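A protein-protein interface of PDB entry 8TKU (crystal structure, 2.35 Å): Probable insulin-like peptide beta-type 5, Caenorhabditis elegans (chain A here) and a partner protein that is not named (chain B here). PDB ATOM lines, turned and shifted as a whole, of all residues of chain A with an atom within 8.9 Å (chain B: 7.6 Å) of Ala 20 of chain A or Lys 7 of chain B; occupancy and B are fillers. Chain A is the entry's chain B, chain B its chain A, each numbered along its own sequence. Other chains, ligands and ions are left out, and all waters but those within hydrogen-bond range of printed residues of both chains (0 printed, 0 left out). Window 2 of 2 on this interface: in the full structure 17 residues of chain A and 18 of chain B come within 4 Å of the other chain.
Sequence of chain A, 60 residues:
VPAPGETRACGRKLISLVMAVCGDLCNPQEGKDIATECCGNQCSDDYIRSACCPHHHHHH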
ATOM      1  N   LYS A  13      30.432 -14.783   4.921  1.00  0.00           N
ATOM      2  CA  LYS A  13      31.017 -14.983   3.597  1.00  0.00           C
ATOM      3  C   LYS A  13      31.358 -16.443   3.342  1.00  0.00           C
ATOM      4  O   LYS A  13      31.097 -16.958   2.251  1.00  0.00           O
ATOM      5  CB  LYS A  13      32.259 -14.109   3.413  1.00  0.00           C
ATOM      6  CG  LYS A  13      31.961 -12.615   3.435  1.00  0.00           C
ATOM      7  CD  LYS A  13      30.918 -12.259   2.390  1.00  0.00           C
ATOM      8  CE  LYS A  13      30.453 -10.843   2.592  1.00  0.00           C
ATOM      9  NZ  LYS A  13      29.224 -10.591   1.815  1.00  0.00           N
ATOM     10  N   LEU A  14      31.937 -17.128   4.324  1.00  0.00           N
ATOM     11  CA  LEU A  14      32.258 -18.541   4.144  1.00  0.00           C
ATOM     12  C   LEU A  14      30.993 -19.369   3.959  1.00  0.00           C
ATOM     13  O   LEU A  14      30.944 -20.290   3.133  1.00  0.00           O
ATOM     14  CB  LEU A  14      33.042 -19.054   5.348  1.00  0.00           C
ATOM     15  CG  LEU A  14      34.541 -19.121   5.148  1.00  0.00           C
ATOM     16  CD1 LEU A  14      35.038 -17.696   5.027  1.00  0.00           C
ATOM     17  CD2 LEU A  14      35.142 -19.772   6.361  1.00  0.00           C
ATOM     18  N   ILE A  15      29.962 -19.066   4.733  1.00  0.00           N
ATOM     19  CA  ILE A  15      28.759 -19.864   4.641  1.00  0.00           C
ATOM     20  C   ILE A  15      28.115 -19.656   3.277  1.00  0.00           C
ATOM     21  O   ILE A  15      27.642 -20.613   2.658  1.00  0.00           O
ATOM     22  CB  ILE A  15      27.824 -19.539   5.824  1.00  0.00           C
ATOM     23  CG1 ILE A  15      26.934 -20.721   6.142  1.00  0.00           C
ATOM     24  CG2 ILE A  15      26.928 -18.343   5.542  1.00  0.00           C
ATOM     25  CD1 ILE A  15      26.129 -20.498   7.392  1.00  0.00           C
ATOM     26  N   SER A  16      28.180 -18.435   2.730  1.00  0.00           N
ATOM     27  CA  SER A  16      27.670 -18.257   1.371  1.00  0.00           C
ATOM     28  C   SER A  16      28.480 -19.066   0.372  1.00  0.00           C
ATOM     29  O   SER A  16      27.915 -19.684  -0.538  1.00  0.00           O
ATOM     30  CB  SER A  16      27.650 -16.788   0.960  1.00  0.00           C
ATOM     31  OG  SER A  16      26.817 -16.073   1.831  1.00  0.00           O
ATOM     32  N   LEU A  17      29.803 -19.086   0.532  1.00  0.00           N
ATOM     33  CA  LEU A  17      30.625 -19.860  -0.384  1.00  0.00           C
ATOM     34  C   LEU A  17      30.309 -21.339  -0.269  1.00  0.00           C
ATOM     35  O   LEU A  17      30.159 -22.041  -1.277  1.00  0.00           O
ATOM     36  CB  LEU A  17      32.102 -19.630  -0.093  1.00  0.00           C
ATOM     37  CG  LEU A  17      32.953 -20.458  -1.055  1.00  0.00           C
ATOM     38  CD1 LEU A  17      33.040 -19.737  -2.395  1.00  0.00           C
ATOM     39  CD2 LEU A  17      34.308 -20.789  -0.483  1.00  0.00           C
ATOM     40  N   VAL A  18      30.229 -21.830   0.964  1.00  0.00           N
ATOM     41  CA  VAL A  18      29.996 -23.253   1.187  1.00  0.00           C
ATOM     42  C   VAL A  18      28.641 -23.677   0.627  1.00  0.00           C
ATOM     43  O   VAL A  18      28.534 -24.691  -0.071  1.00  0.00           O
ATOM     44  CB  VAL A  18      30.140 -23.576   2.680  1.00  0.00           C
ATOM     45  CG1 VAL A  18      29.381 -24.828   3.007  1.00  0.00           C
ATOM     46  CG2 VAL A  18      31.626 -23.754   2.995  1.00  0.00           C
ATOM     47  N   MET A  19      27.595 -22.889   0.893  1.00  0.00           N
ATOM     48  CA  MET A  19      26.276 -23.203   0.356  1.00  0.00           C
ATOM     49  C   MET A  19      26.255 -23.111  -1.167  1.00  0.00           C
ATOM     50  O   MET A  19      25.493 -23.829  -1.817  1.00  0.00           O
ATOM     51  CB  MET A  19      25.213 -22.269   0.947  1.00  0.00           C
ATOM     52  CG  MET A  19      25.005 -22.381   2.460  1.00  0.00           C
ATOM     53  SD  MET A  19      24.547 -24.026   3.073  1.00  0.00           S
ATOM     54  CE  MET A  19      22.932 -24.265   2.328  1.00  0.00           C
ATOM     55  N   ALA A  20      27.064 -22.232  -1.762  1.00  0.00           N
ATOM     56  CA  ALA A  20      27.104 -22.176  -3.221  1.00  0.00           C
ATOM     57  C   ALA A  20      27.782 -23.414  -3.793  1.00  0.00           C
ATOM     58  O   ALA A  20      27.357 -23.950  -4.822  1.00  0.00           O
ATOM     59  CB  ALA A  20      27.827 -20.907  -3.682  1.00  0.00           C
ATOM     60  N   VAL A  21      28.803 -23.912  -3.100  1.00  0.00           N
ATOM     61  CA  VAL A  21      29.565 -25.055  -3.584  1.00  0.00           C
ATOM     62  C   VAL A  21      28.755 -26.333  -3.431  1.00  0.00           C
ATOM     63  O   VAL A  21      28.673 -27.144  -4.359  1.00  0.00           O
ATOM     64  CB  VAL A  21      30.919 -25.119  -2.853  1.00  0.00           C
ATOM     65  CG1 VAL A  21      31.563 -26.478  -2.977  1.00  0.00           C
ATOM     66  CG2 VAL A  21      31.844 -24.068  -3.437  1.00  0.00           C
ATOM     67  N   CYS A  22      28.123 -26.518  -2.276  1.00  0.00           N
ATOM     68  CA  CYS A  22      27.392 -27.748  -2.009  1.00  0.00           C
ATOM     69  C   CYS A  22      25.943 -27.689  -2.492  1.00  0.00           C
ATOM     70  O   CYS A  22      25.413 -28.692  -2.986  1.00  0.00           O
ATOM     71  CB  CYS A  22      27.443 -28.069  -0.519  1.00  0.00           C
ATOM     72  SG  CYS A  22      29.120 -28.335   0.125  1.00  0.00           S
ATOM     73  N   GLY A  23      25.287 -26.545  -2.358  1.00  0.00           N
ATOM     74  CA  GLY A  23      23.883 -26.451  -2.741  1.00  0.00           C
ATOM     75  C   GLY A  23      23.001 -27.063  -1.674  1.00  0.00           C
ATOM     76  O   GLY A  23      23.114 -26.726  -0.488  1.00  0.00           O
ATOM     77  N   ASP A  24      22.091 -27.951  -2.095  1.00  0.00           N
ATOM     78  CA  ASP A  24      21.200 -28.624  -1.152  1.00  0.00           C
ATOM     79  C   ASP A  24      21.925 -29.653  -0.286  1.00  0.00           C
ATOM     80  O   ASP A  24      21.393 -30.048   0.759  1.00  0.00           O
ATOM     81  CB  ASP A  24      20.043 -29.292  -1.901  1.00  0.00           C
ATOM     82  N   LEU A  25      23.117 -30.100  -0.701  1.00  0.00           N
ATOM     83  CA  LEU A  25      23.877 -31.128   0.010  1.00  0.00           C
ATOM     84  C   LEU A  25      24.413 -30.673   1.366  1.00  0.00           C
ATOM     85  O   LEU A  25      24.922 -31.518   2.114  1.00  0.00           O
ATOM     86  CB  LEU A  25      25.070 -31.592  -0.832  1.00  0.00           C
ATOM     87  CG  LEU A  25      24.907 -32.126  -2.252  1.00  0.00           C
ATOM     88  CD1 LEU A  25      26.277 -32.324  -2.899  1.00  0.00           C
ATOM     89  CD2 LEU A  25      24.162 -33.436  -2.183  1.00  0.00           C
ATOM     90  N   CYS A  26      24.293 -29.391   1.719  1.00  0.00           N
ATOM     91  CA  CYS A  26      24.936 -28.853   2.911  1.00  0.00           C
ATOM     92  C   CYS A  26      23.887 -28.433   3.931  1.00  0.00           C
ATOM     93  O   CYS A  26      23.100 -27.512   3.682  1.00  0.00           O
ATOM     94  CB  CYS A  26      25.831 -27.669   2.550  1.00  0.00           C
ATOM     95  SG  CYS A  26      26.655 -26.837   3.952  1.00  0.00           S
ATOM     96  N   ARG A  49      36.112 -25.988   0.735  1.00  0.00           N
ATOM     97  CA  ARG A  49      35.203 -26.347  -0.339  1.00  0.00           C
ATOM     98  C   ARG A  49      34.551 -27.717  -0.144  1.00  0.00           C
ATOM     99  O   ARG A  49      33.439 -27.932  -0.643  1.00  0.00           O
ATOM    100  CB  ARG A  49      35.926 -26.238  -1.682  1.00  0.00           C
ATOM    101  CG  ARG A  49      35.985 -24.765  -2.166  1.00  0.00           C
ATOM    102  CD  ARG A  49      36.536 -24.586  -3.602  1.00  0.00           C
ATOM    103  NE  ARG A  49      37.890 -25.105  -3.729  1.00  0.00           N
ATOM    104  CZ  ARG A  49      38.184 -26.325  -4.151  1.00  0.00           C
ATOM    105  NH1 ARG A  49      37.240 -27.166  -4.542  1.00  0.00           N
ATOM    106  NH2 ARG A  49      39.453 -26.723  -4.152  1.00  0.00           N
ATOM    107  N   CYS A  52      31.594 -29.405   3.924  1.00  0.00           N
ATOM    108  CA  CYS A  52      30.163 -29.607   4.092  1.00  0.00           C
ATOM    109  C   CYS A  52      29.578 -30.622   3.122  1.00  0.00           C
ATOM    110  O   CYS A  52      28.412 -30.987   3.278  1.00  0.00           O
ATOM    111  CB  CYS A  52      29.405 -28.283   3.931  1.00  0.00           C
ATOM    112  SG  CYS A  52      27.827 -28.266   4.822  1.00  0.00           S
ATOM    113  N   CYS A  53      30.351 -31.117   2.156  1.00  0.00           N
ATOM    114  CA  CYS A  53      29.805 -32.098   1.218  1.00  0.00           C
ATOM    115  C   CYS A  53      30.905 -32.930   0.569  1.00  0.00           C
ATOM    116  O   CYS A  53      31.099 -32.848  -0.649  1.00  0.00           O
ATOM    117  CB  CYS A  53      28.976 -31.400   0.135  1.00  0.00           C
ATOM    118  SG  CYS A  53      29.797 -30.023  -0.767  1.00  0.00           S
ATOM    119  N   LYS B   5      34.819 -24.127 -12.022  1.00  0.00           N
ATOM    120  CA  LYS B   5      33.436 -24.265 -11.634  1.00  0.00           C
ATOM    121  C   LYS B   5      32.844 -22.864 -11.674  1.00  0.00           C
ATOM    122  O   LYS B   5      33.526 -21.886 -11.350  1.00  0.00           O
ATOM    123  CB  LYS B   5      33.314 -24.898 -10.238  1.00  0.00           C
ATOM    124  N   ILE B   6      31.610 -22.753 -12.145  1.00  0.00           N
ATOM    125  CA  ILE B   6      30.886 -21.488 -12.147  1.00  0.00           C
ATOM    126  C   ILE B   6      29.425 -21.788 -11.872  1.00  0.00           C
ATOM    127  O   ILE B   6      28.866 -22.729 -12.435  1.00  0.00           O
ATOM    128  CB  ILE B   6      31.056 -20.716 -13.467  1.00  0.00           C
ATOM    129  CG1 ILE B   6      30.563 -19.276 -13.289  1.00  0.00           C
ATOM    130  CG2 ILE B   6      30.413 -21.478 -14.676  1.00  0.00           C
ATOM    131  CD1 ILE B   6      30.969 -18.336 -14.392  1.00  0.00           C
ATOM    132  N   LYS B   7      28.790 -20.971 -11.045  1.00  0.00           N
ATOM    133  CA  LYS B   7      27.471 -21.321 -10.552  1.00  0.00           C
ATOM    134  C   LYS B   7      26.695 -20.054 -10.223  1.00  0.00           C
ATOM    135  O   LYS B   7      27.242 -19.151  -9.587  1.00  0.00           O
ATOM    136  CB  LYS B   7      27.645 -22.239  -9.336  1.00  0.00           C
ATOM    137  CG  LYS B   7      26.368 -22.851  -8.821  1.00  0.00           C
ATOM    138  CD  LYS B   7      26.670 -23.927  -7.780  1.00  0.00           C
ATOM    139  CE  LYS B   7      27.587 -25.011  -8.372  1.00  0.00           C
ATOM    140  NZ  LYS B   7      27.620 -26.286  -7.582  1.00  0.00           N
ATOM    141  N   ILE B   8      25.476 -19.933 -10.755  1.00  0.00           N
ATOM    142  CA  ILE B   8      24.573 -18.849 -10.346  1.00  0.00           C
ATOM    143  C   ILE B   8      24.006 -19.131  -8.961  1.00  0.00           C
ATOM    144  O   ILE B   8      23.604 -20.255  -8.660  1.00  0.00           O
ATOM    145  CB  ILE B   8      23.442 -18.640 -11.362  1.00  0.00           C
ATOM    146  CG1 ILE B   8      23.991 -18.334 -12.753  1.00  0.00           C
ATOM    147  CG2 ILE B   8      22.545 -17.506 -10.928  1.00  0.00           C
ATOM    148  CD1 ILE B   8      24.188 -16.888 -13.002  1.00  0.00           C
ATOM    149  N   VAL B   9      23.915 -18.100  -8.123  1.00  0.00           N
ATOM    150  CA  VAL B   9      23.331 -18.314  -6.806  1.00  0.00           C
ATOM    151  C   VAL B   9      21.806 -18.293  -6.856  1.00  0.00           C
ATOM    152  O   VAL B   9      21.146 -19.086  -6.166  1.00  0.00           O
ATOM    153  CB  VAL B   9      23.868 -17.276  -5.809  1.00  0.00           C
ATOM    154  CG1 VAL B   9      22.985 -17.260  -4.581  1.00  0.00           C
ATOM    155  CG2 VAL B   9      25.345 -17.591  -5.429  1.00  0.00           C
ATOM    156  N   ALA B  10      21.211 -17.391  -7.643  1.00  0.00           N
ATOM    157  CA  ALA B  10      19.751 -17.347  -7.754  1.00  0.00           C
ATOM    158  C   ALA B  10      19.325 -16.758  -9.089  1.00  0.00           C
ATOM    159  O   ALA B  10      19.498 -15.544  -9.285  1.00  0.00           O
ATOM    160  CB  ALA B  10      19.128 -16.540  -6.618  1.00  0.00           C
ATOM    161  N   ASP B  28      24.259 -13.086  -8.350  1.00  0.00           N
ATOM    162  CA  ASP B  28      25.478 -13.458  -7.659  1.00  0.00           C
ATOM    163  C   ASP B  28      25.981 -14.736  -8.295  1.00  0.00           C
ATOM    164  O   ASP B  28      25.194 -15.663  -8.536  1.00  0.00           O
ATOM    165  CB  ASP B  28      25.233 -13.661  -6.163  1.00  0.00           C
ATOM    166  CG  ASP B  28      24.875 -12.357  -5.438  1.00  0.00           C
ATOM    167  OD1 ASP B  28      23.908 -11.684  -5.855  1.00  0.00           O
ATOM    168  OD2 ASP B  28      25.559 -12.008  -4.441  1.00  0.00           O
ATOM    169  N   ILE B  29      27.279 -14.786  -8.566  1.00  0.00           N
ATOM    170  CA  ILE B  29      27.907 -15.913  -9.239  1.00  0.00           C
ATOM    171  C   ILE B  29      29.113 -16.378  -8.441  1.00  0.00           C
ATOM    172  O   ILE B  29      29.994 -15.576  -8.104  1.00  0.00           O
ATOM    173  CB  ILE B  29      28.312 -15.563 -10.681  1.00  0.00           C
ATOM    174  CG1 ILE B  29      27.042 -15.490 -11.533  1.00  0.00           C
ATOM    175  CG2 ILE B  29      29.335 -16.567 -11.194  1.00  0.00           C
ATOM    176  CD1 ILE B  29      27.215 -15.082 -12.940  1.00  0.00           C
ATOM    177  N   MET B  30      29.139 -17.672  -8.142  1.00  0.00           N
ATOM    178  CA  MET B  30      30.268 -18.333  -7.515  1.00  0.00           C
ATOM    179  C   MET B  30      31.127 -18.892  -8.624  1.00  0.00           C
ATOM    180  O   MET B  30      30.601 -19.493  -9.558  1.00  0.00           O
ATOM    181  CB  MET B  30      29.751 -19.455  -6.616  1.00  0.00           C
ATOM    182  CG  MET B  30      30.770 -20.346  -5.920  1.00  0.00           C
ATOM    183  SD  MET B  30      31.405 -21.715  -6.885  1.00  0.00           S
ATOM    184  CE  MET B  30      33.160 -21.321  -6.931  1.00  0.00           C
ATOM    185  N   SER B  31      32.444 -18.740  -8.517  1.00  0.00           N
ATOM    186  CA  SER B  31      33.235 -19.158  -9.671  1.00  0.00           C
ATOM    187  C   SER B  31      34.687 -19.403  -9.286  1.00  0.00           C
ATOM    188  O   SER B  31      35.226 -18.756  -8.386  1.00  0.00           O
ATOM    189  CB  SER B  31      33.158 -18.118 -10.792  1.00  0.00           C
ATOM    190  OG  SER B  31      34.005 -18.468 -11.876  1.00  0.00           O
ATOM    191  N   THR B  32      35.306 -20.337  -9.996  1.00  0.00           N
ATOM    192  CA  THR B  32      36.727 -20.655  -9.947  1.00  0.00           C
ATOM    193  C   THR B  32      37.213 -20.857 -11.369  1.00  0.00           C
ATOM    194  O   THR B  32      36.717 -21.761 -12.040  1.00  0.00           O
ATOM    195  CB  THR B  32      36.981 -21.941  -9.155  1.00  0.00           C
ATOM    196  OG1 THR B  32      36.233 -21.910  -7.937  1.00  0.00           O
ATOM    197  CG2 THR B  32      38.459 -22.093  -8.823  1.00  0.00           C
ATOM    198  N   ALA B  35      35.215 -14.801 -11.826  1.00  0.00           N
ATOM    199  CA  ALA B  35      34.312 -14.543 -12.923  1.00  0.00           C
ATOM    200  C   ALA B  35      34.090 -13.055 -13.071  1.00  0.00           C
ATOM    201  O   ALA B  35      34.073 -12.308 -12.091  1.00  0.00           O
ATOM    202  CB  ALA B  35      32.960 -15.242 -12.737  1.00  0.00           C
ATOM    203  N   GLY B  69      35.543 -17.783  -5.234  1.00  0.00           N
ATOM    204  CA  GLY B  69      34.691 -16.903  -4.468  1.00  0.00           C
ATOM    205  C   GLY B  69      33.433 -16.573  -5.245  1.00  0.00           C
ATOM    206  O   GLY B  69      33.098 -17.222  -6.234  1.00  0.00           O
ATOM    207  N   ILE B  70      32.740 -15.550  -4.752  1.00  0.00           N
ATOM    208  CA  ILE B  70      31.474 -15.093  -5.301  1.00  0.00           C
ATOM    209  C   ILE B  70      31.622 -13.642  -5.722  1.00  0.00           C
ATOM    210  O   ILE B  70      32.159 -12.830  -4.968  1.00  0.00           O
ATOM    211  CB  ILE B  70      30.339 -15.242  -4.275  1.00  0.00           C
ATOM    212  CG1 ILE B  70      30.037 -16.717  -4.019  1.00  0.00           C
ATOM    213  CG2 ILE B  70      29.130 -14.501  -4.728  1.00  0.00           C
ATOM    214  CD1 ILE B  70      29.150 -16.928  -2.786  1.00  0.00           C
ATOM    215  N   VAL B  71      31.164 -13.330  -6.922  1.00  0.00           N
ATOM    216  CA  VAL B  71      31.083 -11.962  -7.412  1.00  0.00           C
ATOM    217  C   VAL B  71      29.600 -11.610  -7.538  1.00  0.00           C
ATOM    218  O   VAL B  71      28.750 -12.490  -7.725  1.00  0.00           O
ATOM    219  CB  VAL B  71      31.843 -11.799  -8.757  1.00  0.00           C
ATOM    220  CG1 VAL B  71      33.366 -12.044  -8.589  1.00  0.00           C
ATOM    221  CG2 VAL B  71      31.299 -12.746  -9.811  1.00  0.00           C
ATOM    222  N   ASN B  94      34.346 -16.886 -16.863  1.00  0.00           N
ATOM    223  CA  ASN B  94      35.625 -17.037 -16.184  1.00  0.00           C
ATOM    224  C   ASN B  94      36.734 -17.501 -17.124  1.00  0.00           C
ATOM    225  O   ASN B  94      37.733 -18.046 -16.662  1.00  0.00           O
ATOM    226  CB  ASN B  94      35.510 -17.980 -14.970  1.00  0.00           C
ATOM    227  CG  ASN B  94      35.189 -19.434 -15.338  1.00  0.00           C
ATOM    228  OD1 ASN B  94      35.327 -19.860 -16.485  1.00  0.00           O
ATOM    229  ND2 ASN B  94      34.753 -20.203 -14.336  1.00  0.00           N
ATOM    230  N   GLN B  97      34.458 -21.164 -18.710  1.00  0.00           N
ATOM    231  CA  GLN B  97      33.057 -21.482 -18.612  1.00  0.00           C
ATOM    232  C   GLN B  97      32.249 -20.207 -18.681  1.00  0.00           C
ATOM    233  O   GLN B  97      32.724 -19.134 -18.282  1.00  0.00           O
ATOM    234  CB  GLN B  97      32.735 -22.190 -17.304  1.00  0.00           C
ATOM    235  CG  GLN B  97      33.569 -23.401 -17.038  1.00  0.00           C
ATOM    236  CD  GLN B  97      33.517 -23.812 -15.594  1.00  0.00           C
ATOM    237  OE1 GLN B  97      33.834 -23.037 -14.691  1.00  0.00           O
ATOM    238  NE2 GLN B  97      32.984 -25.008 -15.359  1.00  0.00           N
ATOM    239  N   ILE B  99      28.024 -18.946 -17.911  1.00  0.00           N
ATOM    240  CA  ILE B  99      26.698 -19.242 -17.410  1.00  0.00           C
ATOM    241  C   ILE B  99      25.824 -18.018 -17.632  1.00  0.00           C
ATOM    242  O   ILE B  99      26.285 -16.878 -17.524  1.00  0.00           O
ATOM    243  CB  ILE B  99      26.736 -19.661 -15.934  1.00  0.00           C
ATOM    244  CG1 ILE B  99      25.365 -20.251 -15.538  1.00  0.00           C
ATOM    245  CG2 ILE B  99      27.145 -18.483 -15.062  1.00  0.00           C
ATOM    246  CD1 ILE B  99      25.465 -21.247 -14.410  1.00  0.00           C
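O of Ser 16 of chain A touches CD1 of Ile 70 of chain B (3.8 Å). Gly 69 of chain B touches Leu 17 of chain A. Ala 20 of chain A touches Lys 7 of chain B. CG of Met 30 of chain B touches CB of Ala 20 of chain A, 3.7 Å away.
Of the 18 printed residues of chain B, 4 touch a printed residue of chain A. Printed residues of chain B that touch a printed residue of chain A: Lys 7, Met 30, Gly 69 and Ile 70. Hydrophobic or aromatic side chains of chain B within 4 Å of the printed part of chain A: Met 30 and Ile 70. Of the 17 printed residues of chain A, 4 touch a printed residue of chain B. Among the printed residues, no Asp or Glu carboxylate lies within 4 Å of a Lys or Arg side-chain nitrogen of the other chain.
Of chain B, only Lys 7 (3.0 Å) and Met 30 (3.7 Å) come within 4 Å of Ala 20 of chain A. Of chain A, only Ala 20 and Val 21 come within 4 Å of Lys 7 of chain B. No residue of chain A comes within 4 Å of Ile 6 of chain B. Printed residues of chain B within 4 Å of Ser 16 of chain A: Ile 70. Of the printed residues of chain B, Leu 17 of chain A touches Gly 69 (3.9 Å). Printed residues of chain B within 4 Å of Val 21 of chain A: Lys 7. Asn 94 of chain B touches none of the printed residues of chain A.
The backbone NH (N) of Lys 7 of chain B sits at hydrogen-bond distance from the backbone carbonyl oxygen (O) of Met 30 of chain B, at 2.8 Å. N of Ser 31 of chain B is in hydrogen-bond range of O of Gly 69 of chain B, 2.8 Å away. SG of Cys 22 of chain A is disulfide-bonded to SG of Cys 53 of chain A (2.0 Å). The side-chain sulfur (SG) of Cys 26 of chain A is disulfide-bonded to the side-chain sulfur (SG) of Cys 52 of chain A (2.0 Å).
The backbone carbonyl oxygen (O) of Val 21 of chain A lies within hydrogen-bond range of the side-chain amino group (NZ) of Lys 7 of chain B (3.5 Å).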
